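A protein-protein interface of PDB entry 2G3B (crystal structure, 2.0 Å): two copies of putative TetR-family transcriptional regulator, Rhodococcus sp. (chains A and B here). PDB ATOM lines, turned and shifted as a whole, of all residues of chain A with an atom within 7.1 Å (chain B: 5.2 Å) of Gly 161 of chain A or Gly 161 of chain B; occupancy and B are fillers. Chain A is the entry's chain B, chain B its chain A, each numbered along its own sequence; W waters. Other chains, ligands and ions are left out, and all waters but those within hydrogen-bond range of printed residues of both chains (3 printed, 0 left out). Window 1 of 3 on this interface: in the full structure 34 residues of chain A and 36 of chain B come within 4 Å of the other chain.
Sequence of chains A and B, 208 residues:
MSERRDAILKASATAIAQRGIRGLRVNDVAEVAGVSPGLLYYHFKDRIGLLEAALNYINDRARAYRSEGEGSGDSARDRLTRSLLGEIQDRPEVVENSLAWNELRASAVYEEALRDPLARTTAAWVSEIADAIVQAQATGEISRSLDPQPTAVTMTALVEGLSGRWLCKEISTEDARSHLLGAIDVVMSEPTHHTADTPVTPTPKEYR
Ala 157 of chain A touches Leu 162 of chain B, and with the chains exchanged Leu 162 of chain A touches Ala 157 of chain B.
Ala 157 of chain A touches Arg 165 of chain B, and with the chains exchanged Arg 165 of chain A touches Ala 157 of chain B.
Glu 160 of chain A touches Arg 165 of chain B, and with the chains exchanged Arg 165 of chain A touches Glu 160 of chain B.
Gly 161 of chain A touches its own counterpart, Gly 161 of chain B.
Water W3 bridges O of Gly 161 of chain A (2.6 Å) and OE1 of Glu 160 of chain B (2.9 Å).
Water W1 bridges the backbone carbonyl oxygen of Gly 161 of chain B (2.7 Å) and the side-chain carboxylate of Glu 160 of chain A (2.9 Å).
Water W2 bridges O of Arg 105 of chain A (2.8 Å) and O of Gly 164 of chain B (2.9 Å).
NE of Arg 105 of chain A is in salt-bridge range of OE1 of Glu 160 of chain A, at 2.9 Å.
The guanidinium group of Arg 165 of chain B lies within hydrogen-bond range of the side-chain hydroxyl of Thr 156 of chain A.
The backbone NH of Ala 157 of chain A lies close to the guanidinium group of Arg 165 of chain B.
OE2 of Glu 160 of chain B lies within salt-bridge range of NH2 of Arg 165 of chain A.
The guanidinium group (NH2) of Arg 165 of chain A lies close to the backbone NH (N) of Ala 157 of chain B (3.5 Å).
OE2 of Glu 160 of chain A lies within salt-bridge range of NH2 of Arg 165 of chain B, 2.8 Å away.
Among the printed residues, merely in contact across the chains: Ala 157 of chain A with Gly 161 of chain B, Gly 161 of chain A with Ala 157 of chain B, Ala 157 of chain A with Leu 162 of chain B, Leu 162 of chain A with Ala 157 of chain B, Arg 105 of chain A with Arg 165 of chain B, Gly 161 of chain A with Gly 161 of chain B, Leu 158 of chain A with Leu 158 of chain B and Arg 105 of chain A with Gly 164 of chain B.
Of the 14 printed residues of chain A, 8 touch a printed residue of chain B.
Among the printed residues, 13 pairs touch across the chains.
Among the printed residues, Asp or Glu carboxylates within 4 Å of a Lys or Arg side-chain nitrogen of the other chain: Glu 160 of chain A with Arg 165 of chain B and Arg 165 of chain A with Glu 160 of chain B.
Val 159 of chain A touches none of the printed residues of chain B.
Printed residues of chain B within 4 Å of Glu 160 of chain A: Arg 165 (2.8 Å).
Of chain B, only Ala 157 (3.3 Å) and Gly 161 (3.7 Å) come within 4 Å of Gly 161 of chain A.
Of the printed residues of chain A, Ala 157 of chain B touches Gly 161, Leu 162 and Arg 165.
Of chain A, only Ala 157 and Gly 161 come within 4 Å of Gly 161 of chain B.
Ser 163 of chain B touches none of the printed residues of chain A.
The nearest residue of chain A that does not touch Gly 161 of chain B is Glu 160 of chain A (4.4 Å).
The nearest printed residue of chain B that does not touch Arg 105 of chain A is Gly 161 of chain B (5.8 Å).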
ATOM      1  N   ASN A 102      -2.373   5.603   6.748  1.00  0.00           N
ATOM      2  CA  ASN A 102      -2.474   4.127   6.728  1.00  0.00           C
ATOM      3  C   ASN A 102      -3.532   3.634   7.736  1.00  0.00           C
ATOM      4  O   ASN A 102      -4.353   2.708   7.461  1.00  0.00           O
ATOM      5  CB  ASN A 102      -1.097   3.548   7.092  1.00  0.00           C
ATOM      6  CG  ASN A 102      -1.017   2.019   6.972  1.00  0.00           C
ATOM      7  OD1 ASN A 102      -0.954   1.470   5.884  1.00  0.00           O
ATOM      8  ND2 ASN A 102      -1.006   1.344   8.095  1.00  0.00           N
ATOM      9  N   ARG A 105      -7.123   4.623   6.548  1.00  0.00           N
ATOM     10  CA  ARG A 105      -7.549   3.630   5.515  1.00  0.00           C
ATOM     11  C   ARG A 105      -8.000   2.307   6.105  1.00  0.00           C
ATOM     12  O   ARG A 105      -9.037   1.736   5.698  1.00  0.00           O
ATOM     13  CB  ARG A 105      -6.388   3.391   4.506  1.00  0.00           C
ATOM     14  CG  ARG A 105      -6.535   2.098   3.661  1.00  0.00           C
ATOM     15  CD  ARG A 105      -7.792   2.093   2.755  1.00  0.00           C
ATOM     16  NE  ARG A 105      -7.602   3.059   1.661  1.00  0.00           N
ATOM     17  CZ  ARG A 105      -8.560   3.524   0.872  1.00  0.00           C
ATOM     18  NH1 ARG A 105      -9.837   3.164   1.016  1.00  0.00           N
ATOM     19  NH2 ARG A 105      -8.224   4.393  -0.068  1.00  0.00           N
ATOM     20  N   THR A 156      -2.073   3.504  -7.822  1.00  0.00           N
ATOM     21  CA  THR A 156      -2.167   4.071  -6.486  1.00  0.00           C
ATOM     22  C   THR A 156      -2.468   2.996  -5.439  1.00  0.00           C
ATOM     23  O   THR A 156      -2.033   3.108  -4.309  1.00  0.00           O
ATOM     24  CB  THR A 156      -3.178   5.215  -6.380  1.00  0.00           C
ATOM     25  OG1 THR A 156      -4.464   4.743  -6.805  1.00  0.00           O
ATOM     26  CG2 THR A 156      -2.694   6.470  -7.264  1.00  0.00           C
ATOM     27  N   ALA A 157      -3.224   1.975  -5.805  1.00  0.00           N
ATOM     28  CA  ALA A 157      -3.512   0.907  -4.808  1.00  0.00           C
ATOM     29  C   ALA A 157      -2.236   0.180  -4.482  1.00  0.00           C
ATOM     30  O   ALA A 157      -2.043  -0.278  -3.358  1.00  0.00           O
ATOM     31  CB  ALA A 157      -4.565  -0.106  -5.348  1.00  0.00           C
ATOM     32  N   LEU A 158      -1.362   0.031  -5.482  1.00  0.00           N
ATOM     33  CA  LEU A 158      -0.051  -0.572  -5.242  1.00  0.00           C
ATOM     34  C   LEU A 158       0.722   0.232  -4.218  1.00  0.00           C
ATOM     35  O   LEU A 158       1.398  -0.354  -3.343  1.00  0.00           O
ATOM     36  CB  LEU A 158       0.777  -0.707  -6.567  1.00  0.00           C
ATOM     37  CG  LEU A 158       2.274  -1.094  -6.474  1.00  0.00           C
ATOM     38  CD1 LEU A 158       2.453  -2.511  -5.801  1.00  0.00           C
ATOM     39  CD2 LEU A 158       3.058  -1.049  -7.841  1.00  0.00           C
ATOM     40  N   VAL A 159       0.742   1.574  -4.392  1.00  0.00           N
ATOM     41  CA  VAL A 159       1.391   2.475  -3.396  1.00  0.00           C
ATOM     42  C   VAL A 159       0.831   2.190  -2.022  1.00  0.00           C
ATOM     43  O   VAL A 159       1.591   2.035  -1.084  1.00  0.00           O
ATOM     44  CB  VAL A 159       1.176   3.970  -3.723  1.00  0.00           C
ATOM     45  CG1 VAL A 159       1.682   4.890  -2.562  1.00  0.00           C
ATOM     46  CG2 VAL A 159       1.941   4.367  -5.019  1.00  0.00           C
ATOM     47  N   GLU A 160      -0.518   2.160  -1.884  1.00  0.00           N
ATOM     48  CA  GLU A 160      -1.110   1.850  -0.542  1.00  0.00           C
ATOM     49  C   GLU A 160      -0.615   0.504   0.024  1.00  0.00           C
ATOM     50  O   GLU A 160      -0.235   0.425   1.225  1.00  0.00           O
ATOM     51  CB  GLU A 160      -2.665   1.880  -0.568  1.00  0.00           C
ATOM     52  CG  GLU A 160      -3.195   3.288  -1.078  1.00  0.00           C
ATOM     53  CD  GLU A 160      -4.645   3.509  -0.731  1.00  0.00           C
ATOM     54  OE1 GLU A 160      -5.101   2.856   0.216  1.00  0.00           O
ATOM     55  OE2 GLU A 160      -5.352   4.292  -1.418  1.00  0.00           O
ATOM     56  N   GLY A 161      -0.606  -0.534  -0.810  1.00  0.00           N
ATOM     57  CA  GLY A 161      -0.102  -1.859  -0.363  1.00  0.00           C
ATOM     58  C   GLY A 161       1.369  -1.868   0.058  1.00  0.00           C
ATOM     59  O   GLY A 161       1.756  -2.407   1.111  1.00  0.00           O
ATOM     60  N   LEU A 162       2.220  -1.286  -0.780  1.00  0.00           N
ATOM     61  CA  LEU A 162       3.642  -1.218  -0.443  1.00  0.00           C
ATOM     62  C   LEU A 162       3.846  -0.338   0.757  1.00  0.00           C
ATOM     63  O   LEU A 162       4.621  -0.655   1.631  1.00  0.00           O
ATOM     64  CB  LEU A 162       4.445  -0.616  -1.598  1.00  0.00           C
ATOM     65  CG  LEU A 162       4.620  -1.572  -2.791  1.00  0.00           C
ATOM     66  CD1 LEU A 162       5.174  -0.770  -3.932  1.00  0.00           C
ATOM     67  CD2 LEU A 162       5.585  -2.727  -2.361  1.00  0.00           C
ATOM     68  N   SER A 163       3.164   0.792   0.804  1.00  0.00           N
ATOM     69  CA  SER A 163       3.278   1.638   1.996  1.00  0.00           C
ATOM     70  C   SER A 163       2.873   0.890   3.284  1.00  0.00           C
ATOM     71  O   SER A 163       3.463   1.072   4.335  1.00  0.00           O
ATOM     72  CB  SER A 163       2.444   2.916   1.829  1.00  0.00           C
ATOM     73  OG  SER A 163       2.578   3.659   3.019  1.00  0.00           O
ATOM     74  N   GLY A 164       1.848   0.044   3.236  1.00  0.00           N
ATOM     75  CA  GLY A 164       1.492  -0.685   4.470  1.00  0.00           C
ATOM     76  C   GLY A 164       2.629  -1.595   4.927  1.00  0.00           C
ATOM     77  O   GLY A 164       2.876  -1.730   6.139  1.00  0.00           O
ATOM     78  N   ARG A 165       3.332  -2.246   3.987  1.00  0.00           N
ATOM     79  CA  ARG A 165       4.500  -3.051   4.328  1.00  0.00           C
ATOM     80  C   ARG A 165       5.699  -2.256   4.832  1.00  0.00           C
ATOM     81  O   ARG A 165       6.374  -2.677   5.786  1.00  0.00           O
ATOM     82  CB  ARG A 165       4.931  -3.875   3.127  1.00  0.00           C
ATOM     83  CG  ARG A 165       3.842  -4.917   2.792  1.00  0.00           C
ATOM     84  CD  ARG A 165       4.326  -5.837   1.773  1.00  0.00           C
ATOM     85  NE  ARG A 165       3.226  -6.708   1.370  1.00  0.00           N
ATOM     86  CZ  ARG A 165       3.319  -7.619   0.417  1.00  0.00           C
ATOM     87  NH1 ARG A 165       4.482  -7.809  -0.202  1.00  0.00           N
ATOM     88  NH2 ARG A 165       2.253  -8.331   0.101  1.00  0.00           N
ATOM     89  N   TRP A 166       5.916  -1.107   4.207  1.00  0.00           N
ATOM     90  CA  TRP A 166       6.966  -0.158   4.560  1.00  0.00           C
ATOM     91  C   TRP A 166       6.800   0.301   6.012  1.00  0.00           C
ATOM     92  O   TRP A 166       7.761   0.340   6.825  1.00  0.00           O
ATOM     93  CB  TRP A 166       6.875   1.044   3.576  1.00  0.00           C
ATOM     94  CG  TRP A 166       7.793   2.199   3.870  1.00  0.00           C
ATOM     95  CD1 TRP A 166       9.156   2.164   4.029  1.00  0.00           C
ATOM     96  CD2 TRP A 166       7.391   3.549   4.105  1.00  0.00           C
ATOM     97  NE1 TRP A 166       9.626   3.438   4.366  1.00  0.00           N
ATOM     98  CE2 TRP A 166       8.565   4.299   4.399  1.00  0.00           C
ATOM     99  CE3 TRP A 166       6.157   4.212   4.056  1.00  0.00           C
ATOM    100  CZ2 TRP A 166       8.532   5.669   4.644  1.00  0.00           C
ATOM    101  CZ3 TRP A 166       6.122   5.591   4.320  1.00  0.00           C
ATOM    102  CH2 TRP A 166       7.305   6.297   4.597  1.00  0.00           C
ATOM    103  N   ILE A 171       9.608  -3.834   4.489  1.00  0.00           N
ATOM    104  CA  ILE A 171      10.377  -3.477   3.290  1.00  0.00           C
ATOM    105  C   ILE A 171      11.046  -2.098   3.510  1.00  0.00           C
ATOM    106  O   ILE A 171      10.459  -1.209   4.131  1.00  0.00           O
ATOM    107  CB  ILE A 171       9.454  -3.517   2.017  1.00  0.00           C
ATOM    108  CG1 ILE A 171      10.201  -3.215   0.724  1.00  0.00           C
ATOM    109  CG2 ILE A 171       8.252  -2.576   2.128  1.00  0.00           C
ATOM    110  CD1 ILE A 171       9.264  -3.314  -0.488  1.00  0.00           C
ATOM    111  N   ALA B 157       1.606  -7.000  -3.034  1.00  0.00           N
ATOM    112  CA  ALA B 157       1.331  -5.685  -2.434  1.00  0.00           C
ATOM    113  C   ALA B 157       0.119  -5.000  -3.104  1.00  0.00           C
ATOM    114  O   ALA B 157      -0.707  -4.352  -2.431  1.00  0.00           O
ATOM    115  CB  ALA B 157       2.582  -4.767  -2.477  1.00  0.00           C
ATOM    116  N   LEU B 158       0.024  -5.120  -4.426  1.00  0.00           N
ATOM    117  CA  LEU B 158      -1.153  -4.648  -5.197  1.00  0.00           C
ATOM    118  C   LEU B 158      -2.467  -5.309  -4.725  1.00  0.00           C
ATOM    119  O   LEU B 158      -3.470  -4.639  -4.483  1.00  0.00           O
ATOM    120  CB  LEU B 158      -0.962  -4.861  -6.733  1.00  0.00           C
ATOM    121  CG  LEU B 158      -2.200  -4.559  -7.600  1.00  0.00           C
ATOM    122  CD1 LEU B 158      -2.606  -3.002  -7.468  1.00  0.00           C
ATOM    123  CD2 LEU B 158      -2.035  -5.004  -9.078  1.00  0.00           C
ATOM    124  N   VAL B 159      -2.437  -6.610  -4.513  1.00  0.00           N
ATOM    125  CA  VAL B 159      -3.631  -7.293  -3.929  1.00  0.00           C
ATOM    126  C   VAL B 159      -4.013  -6.689  -2.553  1.00  0.00           C
ATOM    127  O   VAL B 159      -5.170  -6.417  -2.292  1.00  0.00           O
ATOM    128  CB  VAL B 159      -3.368  -8.842  -3.780  1.00  0.00           C
ATOM    129  CG1 VAL B 159      -4.452  -9.551  -2.882  1.00  0.00           C
ATOM    130  CG2 VAL B 159      -3.230  -9.496  -5.202  1.00  0.00           C
ATOM    131  N   GLU B 160      -3.022  -6.457  -1.678  1.00  0.00           N
ATOM    132  CA  GLU B 160      -3.326  -5.886  -0.374  1.00  0.00           C
ATOM    133  C   GLU B 160      -3.899  -4.456  -0.482  1.00  0.00           C
ATOM    134  O   GLU B 160      -4.826  -4.108   0.213  1.00  0.00           O
ATOM    135  CB  GLU B 160      -2.026  -5.864   0.474  1.00  0.00           C
ATOM    136  CG  GLU B 160      -1.683  -7.269   1.058  1.00  0.00           C
ATOM    137  CD  GLU B 160      -0.641  -7.156   2.180  1.00  0.00           C
ATOM    138  OE1 GLU B 160      -0.835  -6.347   3.125  1.00  0.00           O
ATOM    139  OE2 GLU B 160       0.373  -7.855   2.131  1.00  0.00           O
ATOM    140  N   GLY B 161      -3.315  -3.637  -1.344  1.00  0.00           N
ATOM    141  CA  GLY B 161      -3.832  -2.266  -1.542  1.00  0.00           C
ATOM    142  C   GLY B 161      -5.238  -2.262  -2.127  1.00  0.00           C
ATOM    143  O   GLY B 161      -6.098  -1.474  -1.667  1.00  0.00           O
ATOM    144  N   LEU B 162      -5.480  -3.096  -3.140  1.00  0.00           N
ATOM    145  CA  LEU B 162      -6.834  -3.186  -3.688  1.00  0.00           C
ATOM    146  C   LEU B 162      -7.801  -3.702  -2.650  1.00  0.00           C
ATOM    147  O   LEU B 162      -8.921  -3.210  -2.584  1.00  0.00           O
ATOM    148  CB  LEU B 162      -6.885  -4.123  -4.899  1.00  0.00           C
ATOM    149  CG  LEU B 162      -6.203  -3.524  -6.158  1.00  0.00           C
ATOM    150  CD1 LEU B 162      -6.035  -4.582  -7.238  1.00  0.00           C
ATOM    151  CD2 LEU B 162      -7.019  -2.338  -6.702  1.00  0.00           C
ATOM    152  N   SER B 163      -7.382  -4.730  -1.899  1.00  0.00           N
ATOM    153  CA  SER B 163      -8.251  -5.316  -0.850  1.00  0.00           C
ATOM    154  C   SER B 163      -8.624  -4.293   0.226  1.00  0.00           C
ATOM    155  O   SER B 163      -9.765  -4.277   0.692  1.00  0.00           O
ATOM    156  CB  SER B 163      -7.578  -6.515  -0.192  1.00  0.00           C
ATOM    157  OG  SER B 163      -7.381  -7.531  -1.207  1.00  0.00           O
ATOM    158  N   GLY B 164      -7.680  -3.418   0.576  1.00  0.00           N
ATOM    159  CA  GLY B 164      -7.966  -2.372   1.580  1.00  0.00           C
ATOM    160  C   GLY B 164      -9.096  -1.469   1.100  1.00  0.00           C
ATOM    161  O   GLY B 164      -9.965  -1.076   1.893  1.00  0.00           O
ATOM    162  N   ARG B 165      -9.088  -1.093  -0.184  1.00  0.00           N
ATOM    163  CA  ARG B 165     -10.156  -0.257  -0.747  1.00  0.00           C
ATOM    164  C   ARG B 165     -11.467  -1.019  -0.899  1.00  0.00           C
ATOM    165  O   ARG B 165     -12.567  -0.494  -0.677  1.00  0.00           O
ATOM    166  CB  ARG B 165      -9.682   0.219  -2.130  1.00  0.00           C
ATOM    167  CG  ARG B 165      -8.516   1.244  -2.024  1.00  0.00           C
ATOM    168  CD  ARG B 165      -8.415   2.035  -3.325  1.00  0.00           C
ATOM    169  NE  ARG B 165      -7.175   2.855  -3.286  1.00  0.00           N
ATOM    170  CZ  ARG B 165      -6.525   3.256  -4.370  1.00  0.00           C
ATOM    171  NH1 ARG B 165      -6.991   2.884  -5.570  1.00  0.00           N
ATOM    172  NH2 ARG B 165      -5.429   4.018  -4.246  1.00  0.00           N
HETATM  173  O   HOH W   1      -5.737   0.050   0.535  1.00  0.00           O
HETATM  174  O   HOH W   2      -8.656  -0.806   4.503  1.00  0.00           O
HETATM  175  O   HOH W   3       0.172  -3.617   2.709  1.00  0.00           O
